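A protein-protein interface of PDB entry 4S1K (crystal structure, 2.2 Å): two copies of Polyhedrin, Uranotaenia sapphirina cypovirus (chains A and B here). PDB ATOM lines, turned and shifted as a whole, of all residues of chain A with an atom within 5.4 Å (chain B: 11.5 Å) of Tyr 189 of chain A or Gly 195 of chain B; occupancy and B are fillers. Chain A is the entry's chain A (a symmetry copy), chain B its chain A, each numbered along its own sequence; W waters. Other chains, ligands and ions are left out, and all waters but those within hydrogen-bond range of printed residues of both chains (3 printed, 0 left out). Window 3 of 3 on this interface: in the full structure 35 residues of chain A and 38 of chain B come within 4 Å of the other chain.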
ATOM      1  N   PHE A  49      20.879  28.172 -20.979  1.00  0.00           N
ATOM      2  CA  PHE A  49      22.083  27.554 -21.470  1.00  0.00           C
ATOM      3  C   PHE A  49      23.077  28.624 -21.814  1.00  0.00           C
ATOM      4  O   PHE A  49      24.203  28.555 -21.336  1.00  0.00           O
ATOM      5  CB  PHE A  49      21.774  26.638 -22.662  1.00  0.00           C
ATOM      6  CG  PHE A  49      20.764  25.562 -22.335  1.00  0.00           C
ATOM      7  CD1 PHE A  49      21.025  24.627 -21.326  1.00  0.00           C
ATOM      8  CD2 PHE A  49      19.556  25.502 -22.976  1.00  0.00           C
ATOM      9  CE1 PHE A  49      20.093  23.657 -20.980  1.00  0.00           C
ATOM     10  CE2 PHE A  49      18.619  24.506 -22.655  1.00  0.00           C
ATOM     11  CZ  PHE A  49      18.879  23.591 -21.642  1.00  0.00           C
ATOM     12  N   VAL A  50      22.686  29.586 -22.646  1.00  0.00           N
ATOM     13  CA  VAL A  50      23.514  30.786 -22.910  1.00  0.00           C
ATOM     14  C   VAL A  50      22.608  31.999 -23.046  1.00  0.00           C
ATOM     15  O   VAL A  50      21.857  32.066 -23.991  1.00  0.00           O
ATOM     16  CB  VAL A  50      24.308  30.711 -24.248  1.00  0.00           C
ATOM     17  CG1 VAL A  50      25.350  31.806 -24.329  1.00  0.00           C
ATOM     18  CG2 VAL A  50      24.940  29.344 -24.434  1.00  0.00           C
ATOM     19  N   MET A 182      28.529  24.479 -15.787  1.00  0.00           N
ATOM     20  CA  MET A 182      28.590  23.018 -15.867  1.00  0.00           C
ATOM     21  C   MET A 182      29.759  22.426 -15.046  1.00  0.00           C
ATOM     22  O   MET A 182      30.285  21.373 -15.373  1.00  0.00           O
ATOM     23  CB  MET A 182      28.687  22.576 -17.337  1.00  0.00           C
ATOM     24  CG  MET A 182      27.681  23.265 -18.235  1.00  0.00           C
ATOM     25  SD  MET A 182      27.709  22.624 -19.924  1.00  0.00           S
ATOM     26  CE  MET A 182      26.474  23.745 -20.576  1.00  0.00           C
ATOM     27  N   ASN A 187      28.933  17.767 -19.456  1.00  0.00           N
ATOM     28  CA  ASN A 187      28.875  18.660 -20.581  1.00  0.00           C
ATOM     29  C   ASN A 187      27.536  18.456 -21.212  1.00  0.00           C
ATOM     30  O   ASN A 187      27.360  17.473 -21.900  1.00  0.00           O
ATOM     31  CB  ASN A 187      29.988  18.366 -21.602  1.00  0.00           C
ATOM     32  CG  ASN A 187      29.895  19.262 -22.839  1.00  0.00           C
ATOM     33  OD1 ASN A 187      28.966  20.071 -22.965  1.00  0.00           O
ATOM     34  ND2 ASN A 187      30.864  19.135 -23.751  1.00  0.00           N
ATOM     35  N   LEU A 188      26.628  19.398 -21.015  1.00  0.00           N
ATOM     36  CA  LEU A 188      25.289  19.358 -21.616  1.00  0.00           C
ATOM     37  C   LEU A 188      25.278  19.373 -23.178  1.00  0.00           C
ATOM     38  O   LEU A 188      24.295  18.981 -23.801  1.00  0.00           O
ATOM     39  CB  LEU A 188      24.463  20.530 -21.076  1.00  0.00           C
ATOM     40  CG  LEU A 188      24.222  20.594 -19.563  1.00  0.00           C
ATOM     41  CD1 LEU A 188      23.363  21.813 -19.227  1.00  0.00           C
ATOM     42  CD2 LEU A 188      23.579  19.305 -19.039  1.00  0.00           C
ATOM     43  N   TYR A 189      26.387  19.802 -23.794  1.00  0.00           N
ATOM     44  CA  TYR A 189      26.555  19.785 -25.250  1.00  0.00           C
ATOM     45  C   TYR A 189      27.004  18.441 -25.838  1.00  0.00           C
ATOM     46  O   TYR A 189      27.059  18.301 -27.048  1.00  0.00           O
ATOM     47  CB  TYR A 189      27.594  20.845 -25.677  1.00  0.00           C
ATOM     48  CG  TYR A 189      27.164  22.253 -25.384  1.00  0.00           C
ATOM     49  CD1 TYR A 189      26.099  22.825 -26.088  1.00  0.00           C
ATOM     50  CD2 TYR A 189      27.782  23.009 -24.374  1.00  0.00           C
ATOM     51  CE1 TYR A 189      25.683  24.120 -25.821  1.00  0.00           C
ATOM     52  CE2 TYR A 189      27.377  24.295 -24.102  1.00  0.00           C
ATOM     53  CZ  TYR A 189      26.325  24.848 -24.826  1.00  0.00           C
ATOM     54  OH  TYR A 189      25.907  26.124 -24.577  1.00  0.00           O
ATOM     55  N   ALA A 190      27.368  17.495 -24.975  1.00  0.00           N
ATOM     56  CA  ALA A 190      27.952  16.246 -25.358  1.00  0.00           C
ATOM     57  C   ALA A 190      26.840  15.240 -25.452  1.00  0.00           C
ATOM     58  O   ALA A 190      25.859  15.270 -24.675  1.00  0.00           O
ATOM     59  CB  ALA A 190      28.974  15.793 -24.295  1.00  0.00           C
ATOM     60  N   GLY A 191      27.012  14.324 -26.393  1.00  0.00           N
ATOM     61  CA  GLY A 191      26.090  13.237 -26.612  1.00  0.00           C
ATOM     62  C   GLY A 191      24.761  13.687 -27.179  1.00  0.00           C
ATOM     63  O   GLY A 191      24.650  14.796 -27.709  1.00  0.00           O
ATOM     64  N   LEU A 194      22.630  17.337 -26.926  1.00  0.00           N
ATOM     65  CA  LEU A 194      22.949  18.523 -27.687  1.00  0.00           C
ATOM     66  C   LEU A 194      21.745  19.056 -28.477  1.00  0.00           C
ATOM     67  O   LEU A 194      21.447  20.240 -28.414  1.00  0.00           O
ATOM     68  CB  LEU A 194      24.128  18.260 -28.602  1.00  0.00           C
ATOM     69  CG  LEU A 194      24.376  19.378 -29.602  1.00  0.00           C
ATOM     70  CD1 LEU A 194      24.911  20.589 -28.864  1.00  0.00           C
ATOM     71  CD2 LEU A 194      25.307  18.893 -30.709  1.00  0.00           C
ATOM     72  N   VAL A 197      19.572  21.028 -26.162  1.00  0.00           N
ATOM     73  CA  VAL A 197      20.182  22.281 -25.708  1.00  0.00           C
ATOM     74  C   VAL A 197      20.045  23.343 -26.806  1.00  0.00           C
ATOM     75  O   VAL A 197      19.586  24.462 -26.548  1.00  0.00           O
ATOM     76  CB  VAL A 197      21.667  22.074 -25.326  1.00  0.00           C
ATOM     77  CG1 VAL A 197      22.352  23.391 -24.997  1.00  0.00           C
ATOM     78  CG2 VAL A 197      21.782  21.154 -24.127  1.00  0.00           C
ATOM     79  N   LEU A 201      18.135  27.350 -26.960  1.00  0.00           N
ATOM     80  CA  LEU A 201      18.860  28.638 -27.110  1.00  0.00           C
ATOM     81  C   LEU A 201      17.968  29.655 -27.761  1.00  0.00           C
ATOM     82  O   LEU A 201      17.263  29.300 -28.722  1.00  0.00           O
ATOM     83  CB  LEU A 201      20.072  28.463 -28.026  1.00  0.00           C
ATOM     84  CG  LEU A 201      21.201  27.622 -27.456  1.00  0.00           C
ATOM     85  CD1 LEU A 201      22.226  27.293 -28.542  1.00  0.00           C
ATOM     86  CD2 LEU A 201      21.849  28.376 -26.312  1.00  0.00           C
ATOM     87  N   TYR B  23      40.986  32.713 -34.244  1.00  0.00           N
ATOM     88  CA  TYR B  23      39.773  32.197 -33.587  1.00  0.00           C
ATOM     89  C   TYR B  23      39.083  33.404 -32.906  1.00  0.00           C
ATOM     90  O   TYR B  23      39.780  34.282 -32.420  1.00  0.00           O
ATOM     91  CB  TYR B  23      40.125  31.073 -32.603  1.00  0.00           C
ATOM     92  CG  TYR B  23      38.909  30.425 -31.977  1.00  0.00           C
ATOM     93  CD1 TYR B  23      38.186  29.446 -32.644  1.00  0.00           C
ATOM     94  CD2 TYR B  23      38.486  30.803 -30.717  1.00  0.00           C
ATOM     95  CE1 TYR B  23      37.062  28.850 -32.060  1.00  0.00           C
ATOM     96  CE2 TYR B  23      37.378  30.213 -30.135  1.00  0.00           C
ATOM     97  CZ  TYR B  23      36.665  29.244 -30.808  1.00  0.00           C
ATOM     98  OH  TYR B  23      35.573  28.693 -30.178  1.00  0.00           O
ATOM     99  N   ASP B  24      37.745  33.486 -32.974  1.00  0.00           N
ATOM    100  CA  ASP B  24      36.945  34.612 -32.434  1.00  0.00           C
ATOM    101  C   ASP B  24      37.098  35.969 -33.156  1.00  0.00           C
ATOM    102  O   ASP B  24      36.473  36.944 -32.749  1.00  0.00           O
ATOM    103  CB  ASP B  24      37.182  34.801 -30.900  1.00  0.00           C
ATOM    104  CG  ASP B  24      36.270  33.924 -30.053  1.00  0.00           C
ATOM    105  OD1 ASP B  24      35.357  33.283 -30.625  1.00  0.00           O
ATOM    106  OD2 ASP B  24      36.453  33.879 -28.814  1.00  0.00           O
ATOM    107  N   ASN B  47      30.307  37.979 -37.256  1.00  0.00           N
ATOM    108  CA  ASN B  47      30.409  36.787 -36.390  1.00  0.00           C
ATOM    109  C   ASN B  47      31.645  35.999 -36.748  1.00  0.00           C
ATOM    110  O   ASN B  47      32.050  36.071 -37.895  1.00  0.00           O
ATOM    111  CB  ASN B  47      29.212  35.848 -36.548  1.00  0.00           C
ATOM    112  CG  ASN B  47      29.120  34.895 -35.421  1.00  0.00           C
ATOM    113  OD1 ASN B  47      29.513  33.737 -35.518  1.00  0.00           O
ATOM    114  ND2 ASN B  47      28.714  35.415 -34.283  1.00  0.00           N
ATOM    115  N   PHE B  49      31.975  32.719 -36.742  1.00  0.00           N
ATOM    116  CA  PHE B  49      31.734  31.324 -37.005  1.00  0.00           C
ATOM    117  C   PHE B  49      30.710  31.201 -38.094  1.00  0.00           C
ATOM    118  O   PHE B  49      30.970  30.505 -39.068  1.00  0.00           O
ATOM    119  CB  PHE B  49      31.313  30.597 -35.721  1.00  0.00           C
ATOM    120  CG  PHE B  49      32.330  30.723 -34.608  1.00  0.00           C
ATOM    121  CD1 PHE B  49      33.635  30.246 -34.782  1.00  0.00           C
ATOM    122  CD2 PHE B  49      32.020  31.346 -33.429  1.00  0.00           C
ATOM    123  CE1 PHE B  49      34.595  30.390 -33.790  1.00  0.00           C
ATOM    124  CE2 PHE B  49      32.975  31.468 -32.408  1.00  0.00           C
ATOM    125  CZ  PHE B  49      34.273  31.007 -32.593  1.00  0.00           C
ATOM    126  N   ASN B 187      37.777  20.836 -37.498  1.00  0.00           N
ATOM    127  CA  ASN B 187      36.369  21.107 -37.386  1.00  0.00           C
ATOM    128  C   ASN B 187      36.168  21.733 -36.044  1.00  0.00           C
ATOM    129  O   ASN B 187      36.175  21.021 -35.061  1.00  0.00           O
ATOM    130  CB  ASN B 187      35.528  19.823 -37.499  1.00  0.00           C
ATOM    131  CG  ASN B 187      34.033  20.087 -37.308  1.00  0.00           C
ATOM    132  OD1 ASN B 187      33.622  21.223 -37.036  1.00  0.00           O
ATOM    133  ND2 ASN B 187      33.211  19.045 -37.464  1.00  0.00           N
ATOM    134  N   LEU B 188      35.943  23.036 -36.015  1.00  0.00           N
ATOM    135  CA  LEU B 188      35.675  23.776 -34.775  1.00  0.00           C
ATOM    136  C   LEU B 188      34.389  23.322 -34.013  1.00  0.00           C
ATOM    137  O   LEU B 188      34.245  23.577 -32.821  1.00  0.00           O
ATOM    138  CB  LEU B 188      35.592  25.273 -35.094  1.00  0.00           C
ATOM    139  CG  LEU B 188      36.832  25.942 -35.700  1.00  0.00           C
ATOM    140  CD1 LEU B 188      36.560  27.430 -35.921  1.00  0.00           C
ATOM    141  CD2 LEU B 188      38.071  25.731 -34.824  1.00  0.00           C
ATOM    142  N   TYR B 189      33.481  22.625 -34.707  1.00  0.00           N
ATOM    143  CA  TYR B 189      32.273  22.055 -34.103  1.00  0.00           C
ATOM    144  C   TYR B 189      32.469  20.700 -33.409  1.00  0.00           C
ATOM    145  O   TYR B 189      31.548  20.206 -32.782  1.00  0.00           O
ATOM    146  CB  TYR B 189      31.180  21.868 -35.178  1.00  0.00           C
ATOM    147  CG  TYR B 189      30.704  23.160 -35.775  1.00  0.00           C
ATOM    148  CD1 TYR B 189      29.971  24.066 -35.001  1.00  0.00           C
ATOM    149  CD2 TYR B 189      31.019  23.511 -37.098  1.00  0.00           C
ATOM    150  CE1 TYR B 189      29.534  25.268 -35.534  1.00  0.00           C
ATOM    151  CE2 TYR B 189      30.589  24.702 -37.638  1.00  0.00           C
ATOM    152  CZ  TYR B 189      29.848  25.579 -36.852  1.00  0.00           C
ATOM    153  OH  TYR B 189      29.407  26.767 -37.366  1.00  0.00           O
ATOM    154  N   ALA B 190      33.645  20.099 -33.577  1.00  0.00           N
ATOM    155  CA  ALA B 190      33.936  18.772 -33.127  1.00  0.00           C
ATOM    156  C   ALA B 190      34.584  18.888 -31.777  1.00  0.00           C
ATOM    157  O   ALA B 190      35.351  19.836 -31.495  1.00  0.00           O
ATOM    158  CB  ALA B 190      34.904  18.082 -34.111  1.00  0.00           C
ATOM    159  N   GLY B 191      34.295  17.897 -30.948  1.00  0.00           N
ATOM    160  CA  GLY B 191      34.857  17.788 -29.624  1.00  0.00           C
ATOM    161  C   GLY B 191      34.344  18.844 -28.669  1.00  0.00           C
ATOM    162  O   GLY B 191      33.313  19.471 -28.925  1.00  0.00           O
ATOM    163  N   PRO B 192      35.096  19.080 -27.572  1.00  0.00           N
ATOM    164  CA  PRO B 192      34.669  20.024 -26.536  1.00  0.00           C
ATOM    165  C   PRO B 192      34.514  21.461 -27.013  1.00  0.00           C
ATOM    166  O   PRO B 192      33.822  22.225 -26.364  1.00  0.00           O
ATOM    167  CB  PRO B 192      35.779  19.946 -25.484  1.00  0.00           C
ATOM    168  CG  PRO B 192      36.487  18.645 -25.735  1.00  0.00           C
ATOM    169  CD  PRO B 192      36.317  18.341 -27.189  1.00  0.00           C
ATOM    170  N   LEU B 193      35.148  21.855 -28.113  1.00  0.00           N
ATOM    171  CA  LEU B 193      35.090  23.285 -28.515  1.00  0.00           C
ATOM    172  C   LEU B 193      33.710  23.728 -28.983  1.00  0.00           C
ATOM    173  O   LEU B 193      33.426  24.935 -29.079  1.00  0.00           O
ATOM    174  CB  LEU B 193      36.096  23.588 -29.616  1.00  0.00           C
ATOM    175  CG  LEU B 193      36.374  25.070 -29.875  1.00  0.00           C
ATOM    176  CD1 LEU B 193      37.062  25.695 -28.668  1.00  0.00           C
ATOM    177  CD2 LEU B 193      37.216  25.153 -31.129  1.00  0.00           C
ATOM    178  N   LEU B 194      32.849  22.759 -29.268  1.00  0.00           N
ATOM    179  CA  LEU B 194      31.520  23.061 -29.750  1.00  0.00           C
ATOM    180  C   LEU B 194      30.760  24.014 -28.817  1.00  0.00           C
ATOM    181  O   LEU B 194      30.200  25.001 -29.274  1.00  0.00           O
ATOM    182  CB  LEU B 194      30.741  21.783 -29.977  1.00  0.00           C
ATOM    183  CG  LEU B 194      29.265  22.019 -30.256  1.00  0.00           C
ATOM    184  CD1 LEU B 194      29.116  22.637 -31.632  1.00  0.00           C
ATOM    185  CD2 LEU B 194      28.487  20.716 -30.100  1.00  0.00           C
ATOM    186  N   GLY B 195      30.719  23.718 -27.525  1.00  0.00           N
ATOM    187  CA  GLY B 195      30.046  24.615 -26.599  1.00  0.00           C
ATOM    188  C   GLY B 195      30.527  26.052 -26.775  1.00  0.00           C
ATOM    189  O   GLY B 195      29.710  26.966 -26.776  1.00  0.00           O
ATOM    190  N   ASN B 196      31.836  26.255 -26.944  1.00  0.00           N
ATOM    191  CA  ASN B 196      32.395  27.613 -27.110  1.00  0.00           C
ATOM    192  C   ASN B 196      31.995  28.288 -28.434  1.00  0.00           C
ATOM    193  O   ASN B 196      31.762  29.474 -28.485  1.00  0.00           O
ATOM    194  CB  ASN B 196      33.931  27.553 -26.945  1.00  0.00           C
ATOM    195  CG  ASN B 196      34.601  28.923 -26.804  1.00  0.00           C
ATOM    196  OD1 ASN B 196      34.733  29.487 -25.708  1.00  0.00           O
ATOM    197  ND2 ASN B 196      35.090  29.419 -27.911  1.00  0.00           N
ATOM    198  N   VAL B 197      31.890  27.511 -29.498  1.00  0.00           N
ATOM    199  CA  VAL B 197      31.475  28.019 -30.809  1.00  0.00           C
ATOM    200  C   VAL B 197      30.007  28.462 -30.745  1.00  0.00           C
ATOM    201  O   VAL B 197      29.668  29.580 -31.151  1.00  0.00           O
ATOM    202  CB  VAL B 197      31.678  26.951 -31.911  1.00  0.00           C
ATOM    203  CG1 VAL B 197      31.114  27.407 -33.247  1.00  0.00           C
ATOM    204  CG2 VAL B 197      33.152  26.645 -32.086  1.00  0.00           C
ATOM    205  N   ILE B 198      29.152  27.598 -30.204  1.00  0.00           N
ATOM    206  CA  ILE B 198      27.716  27.907 -29.966  1.00  0.00           C
ATOM    207  C   ILE B 198      27.495  29.163 -29.131  1.00  0.00           C
ATOM    208  O   ILE B 198      26.606  29.943 -29.418  1.00  0.00           O
ATOM    209  CB  ILE B 198      26.977  26.701 -29.300  1.00  0.00           C
ATOM    210  CG1 ILE B 198      26.879  25.552 -30.298  1.00  0.00           C
ATOM    211  CG2 ILE B 198      25.562  27.089 -28.877  1.00  0.00           C
ATOM    212  CD1 ILE B 198      26.400  24.263 -29.710  1.00  0.00           C
ATOM    213  N   GLU B 199      28.332  29.363 -28.111  1.00  0.00           N
ATOM    214  CA  GLU B 199      28.252  30.549 -27.268  1.00  0.00           C
ATOM    215  C   GLU B 199      28.574  31.842 -28.025  1.00  0.00           C
ATOM    216  O   GLU B 199      28.185  32.918 -27.580  1.00  0.00           O
ATOM    217  CB  GLU B 199      29.165  30.407 -26.058  1.00  0.00           C
ATOM    218  CG  GLU B 199      28.650  29.386 -25.050  1.00  0.00           C
ATOM    219  CD  GLU B 199      29.712  28.939 -24.068  1.00  0.00           C
ATOM    220  OE1 GLU B 199      30.881  29.428 -24.141  1.00  0.00           O
ATOM    221  OE2 GLU B 199      29.365  28.102 -23.205  1.00  0.00           O
ATOM    222  N   GLY B 200      29.312  31.716 -29.123  1.00  0.00           N
ATOM    223  CA  GLY B 200      29.737  32.849 -29.916  1.00  0.00           C
ATOM    224  C   GLY B 200      28.847  33.224 -31.088  1.00  0.00           C
ATOM    225  O   GLY B 200      28.997  34.308 -31.639  1.00  0.00           O
ATOM    226  N   LEU B 201      27.948  32.326 -31.489  1.00  0.00           N
ATOM    227  CA  LEU B 201      27.002  32.591 -32.603  1.00  0.00           C
ATOM    228  C   LEU B 201      26.040  33.675 -32.212  1.00  0.00           C
ATOM    229  O   LEU B 201      25.557  33.656 -31.066  1.00  0.00           O
ATOM    230  CB  LEU B 201      26.167  31.345 -32.900  1.00  0.00           C
ATOM    231  CG  LEU B 201      26.930  30.182 -33.509  1.00  0.00           C
ATOM    232  CD1 LEU B 201      26.068  28.918 -33.511  1.00  0.00           C
ATOM    233  CD2 LEU B 201      27.350  30.551 -34.917  1.00  0.00           C
ATOM    234  N   ASP B 202      25.727  34.599 -33.126  1.00  0.00           N
ATOM    235  CA  ASP B 202      24.653  35.575 -32.862  1.00  0.00           C
ATOM    236  C   ASP B 202      24.918  36.493 -31.614  1.00  0.00           C
ATOM    237  O   ASP B 202      24.022  36.768 -30.810  1.00  0.00           O
ATOM    238  CB  ASP B 202      23.295  34.847 -32.680  1.00  0.00           C
ATOM    239  CG  ASP B 202      23.007  33.770 -33.760  1.00  0.00           C
ATOM    240  OD1 ASP B 202      23.526  33.849 -34.892  1.00  0.00           O
ATOM    241  OD2 ASP B 202      22.226  32.833 -33.464  1.00  0.00           O
ATOM    242  N   THR B 203      26.144  36.974 -31.458  1.00  0.00           N
ATOM    243  CA  THR B 203      26.508  37.782 -30.294  1.00  0.00           C
ATOM    244  C   THR B 203      26.865  39.245 -30.607  1.00  0.00           C
ATOM    245  O   THR B 203      27.122  40.031 -29.694  1.00  0.00           O
ATOM    246  CB  THR B 203      27.714  37.145 -29.584  1.00  0.00           C
ATOM    247  OG1 THR B 203      28.684  36.773 -30.568  1.00  0.00           O
ATOM    248  CG2 THR B 203      27.283  35.885 -28.827  1.00  0.00           C
HETATM  249  O   HOH W   1      31.105  19.271 -27.203  1.00  0.00           O
HETATM  250  O   HOH W   2      27.039  27.296 -22.418  1.00  0.00           O
HETATM  251  O   HOH W   3      31.069  21.380 -25.801  1.00  0.00           O
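The backbone NH (N) of Tyr 189 of chain A lies within hydrogen-bond range of the side-chain amide oxygen (OD1) of Asn 187 of chain A, at 2.7 Å.
Among the printed residues, pairs that only touch across the chains: Val 50 of chain A with Glu 199 of chain B (3.8 Å), Tyr 189 of chain A with Gly 195 of chain B (3.6 Å), Tyr 189 of chain A with Ile 198 of chain B (3.9 Å), Leu 194 of chain A with Leu 194 of chain B (3.7 Å) and Leu 201 of chain A with Ile 198 of chain B (3.4 Å).
Of chain B, only Gly 195 and Ile 198 come within 4 Å of Tyr 189 of chain A. Of chain A, only Tyr 189 (3.6 Å) comes within 4 Å of Gly 195 of chain B. Of the printed residues of chain B, Val 50 of chain A touches Glu 199 (3.8 Å). No residue of chain B comes within 4 Å of Asn 187 of chain A. No residue of chain B comes within 4 Å of Leu 188 of chain A. No residue of chain B comes within 4 Å of Ala 190 of chain A. No residue of chain B comes within 4 Å of Gly 191 of chain A. Leu 194 of chain A touches one residue of chain B. Of the printed residues of chain A, Ile 198 of chain B touches Tyr 189 (3.9 Å) and Leu 201 (3.4 Å). Of the printed residues of chain A, Glu 199 of chain B touches Val 50 (3.8 Å). Of the printed residues of chain A, Leu 194 of chain B touches Leu 194 (3.7 Å). Of the printed residues of chain B, Leu 201 of chain A touches Ile 198 (3.4 Å). The nearest printed residue of chain A that does not touch Gly 195 of chain B is Val 50 of chain A (5.8 Å). The nearest printed residue of chain A that does not touch Ile 198 of chain B is Leu 194 of chain A (4.1 Å).
Hydrophobic or aromatic side chains of chain B within 4 Å of the printed part of chain A: Leu 194 and Ile 198. Of the 11 printed residues of chain A, 4 touch a printed residue of chain B. Along chain A the printed residues that touch a printed residue of chain B span positions 50 to 201. Among the printed residues, no Asp or Glu carboxylate lies within 4 Å of a Lys or Arg side-chain nitrogen of the other chain.
Leu 194 of chain A touches its own counterpart, Leu 194 of chain B. Positions printed for both chains: 49, 187, 188, 189, 190, 191, 194, 197 and 201. Of the 5 pairs that touch across the chains among the printed residues, 1 has its exchanged pair printed and touching as well.
Water W2 lies within hydrogen-bond range of the side-chain carboxylate of Glu 199 of chain B (2.6 Å), the side-chain hydroxyl of Tyr 189 of chain A (2.7 Å) and the backbone carbonyl oxygen of Phe 49 of chain A (3.3 Å). Water W1 bridges O of Gly 191 of chain B (2.8 Å) and ND2 of Asn 187 of chain A (3.5 Å). Water W3 lies within hydrogen-bond range of the backbone NH (N) of Gly 195 of chain B (2.9 Å), the backbone carbonyl oxygen (O) of Pro 192 of chain B (2.9 Å) and the side-chain amide nitrogen (ND2) of Asn 187 of chain A (3.0 Å).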
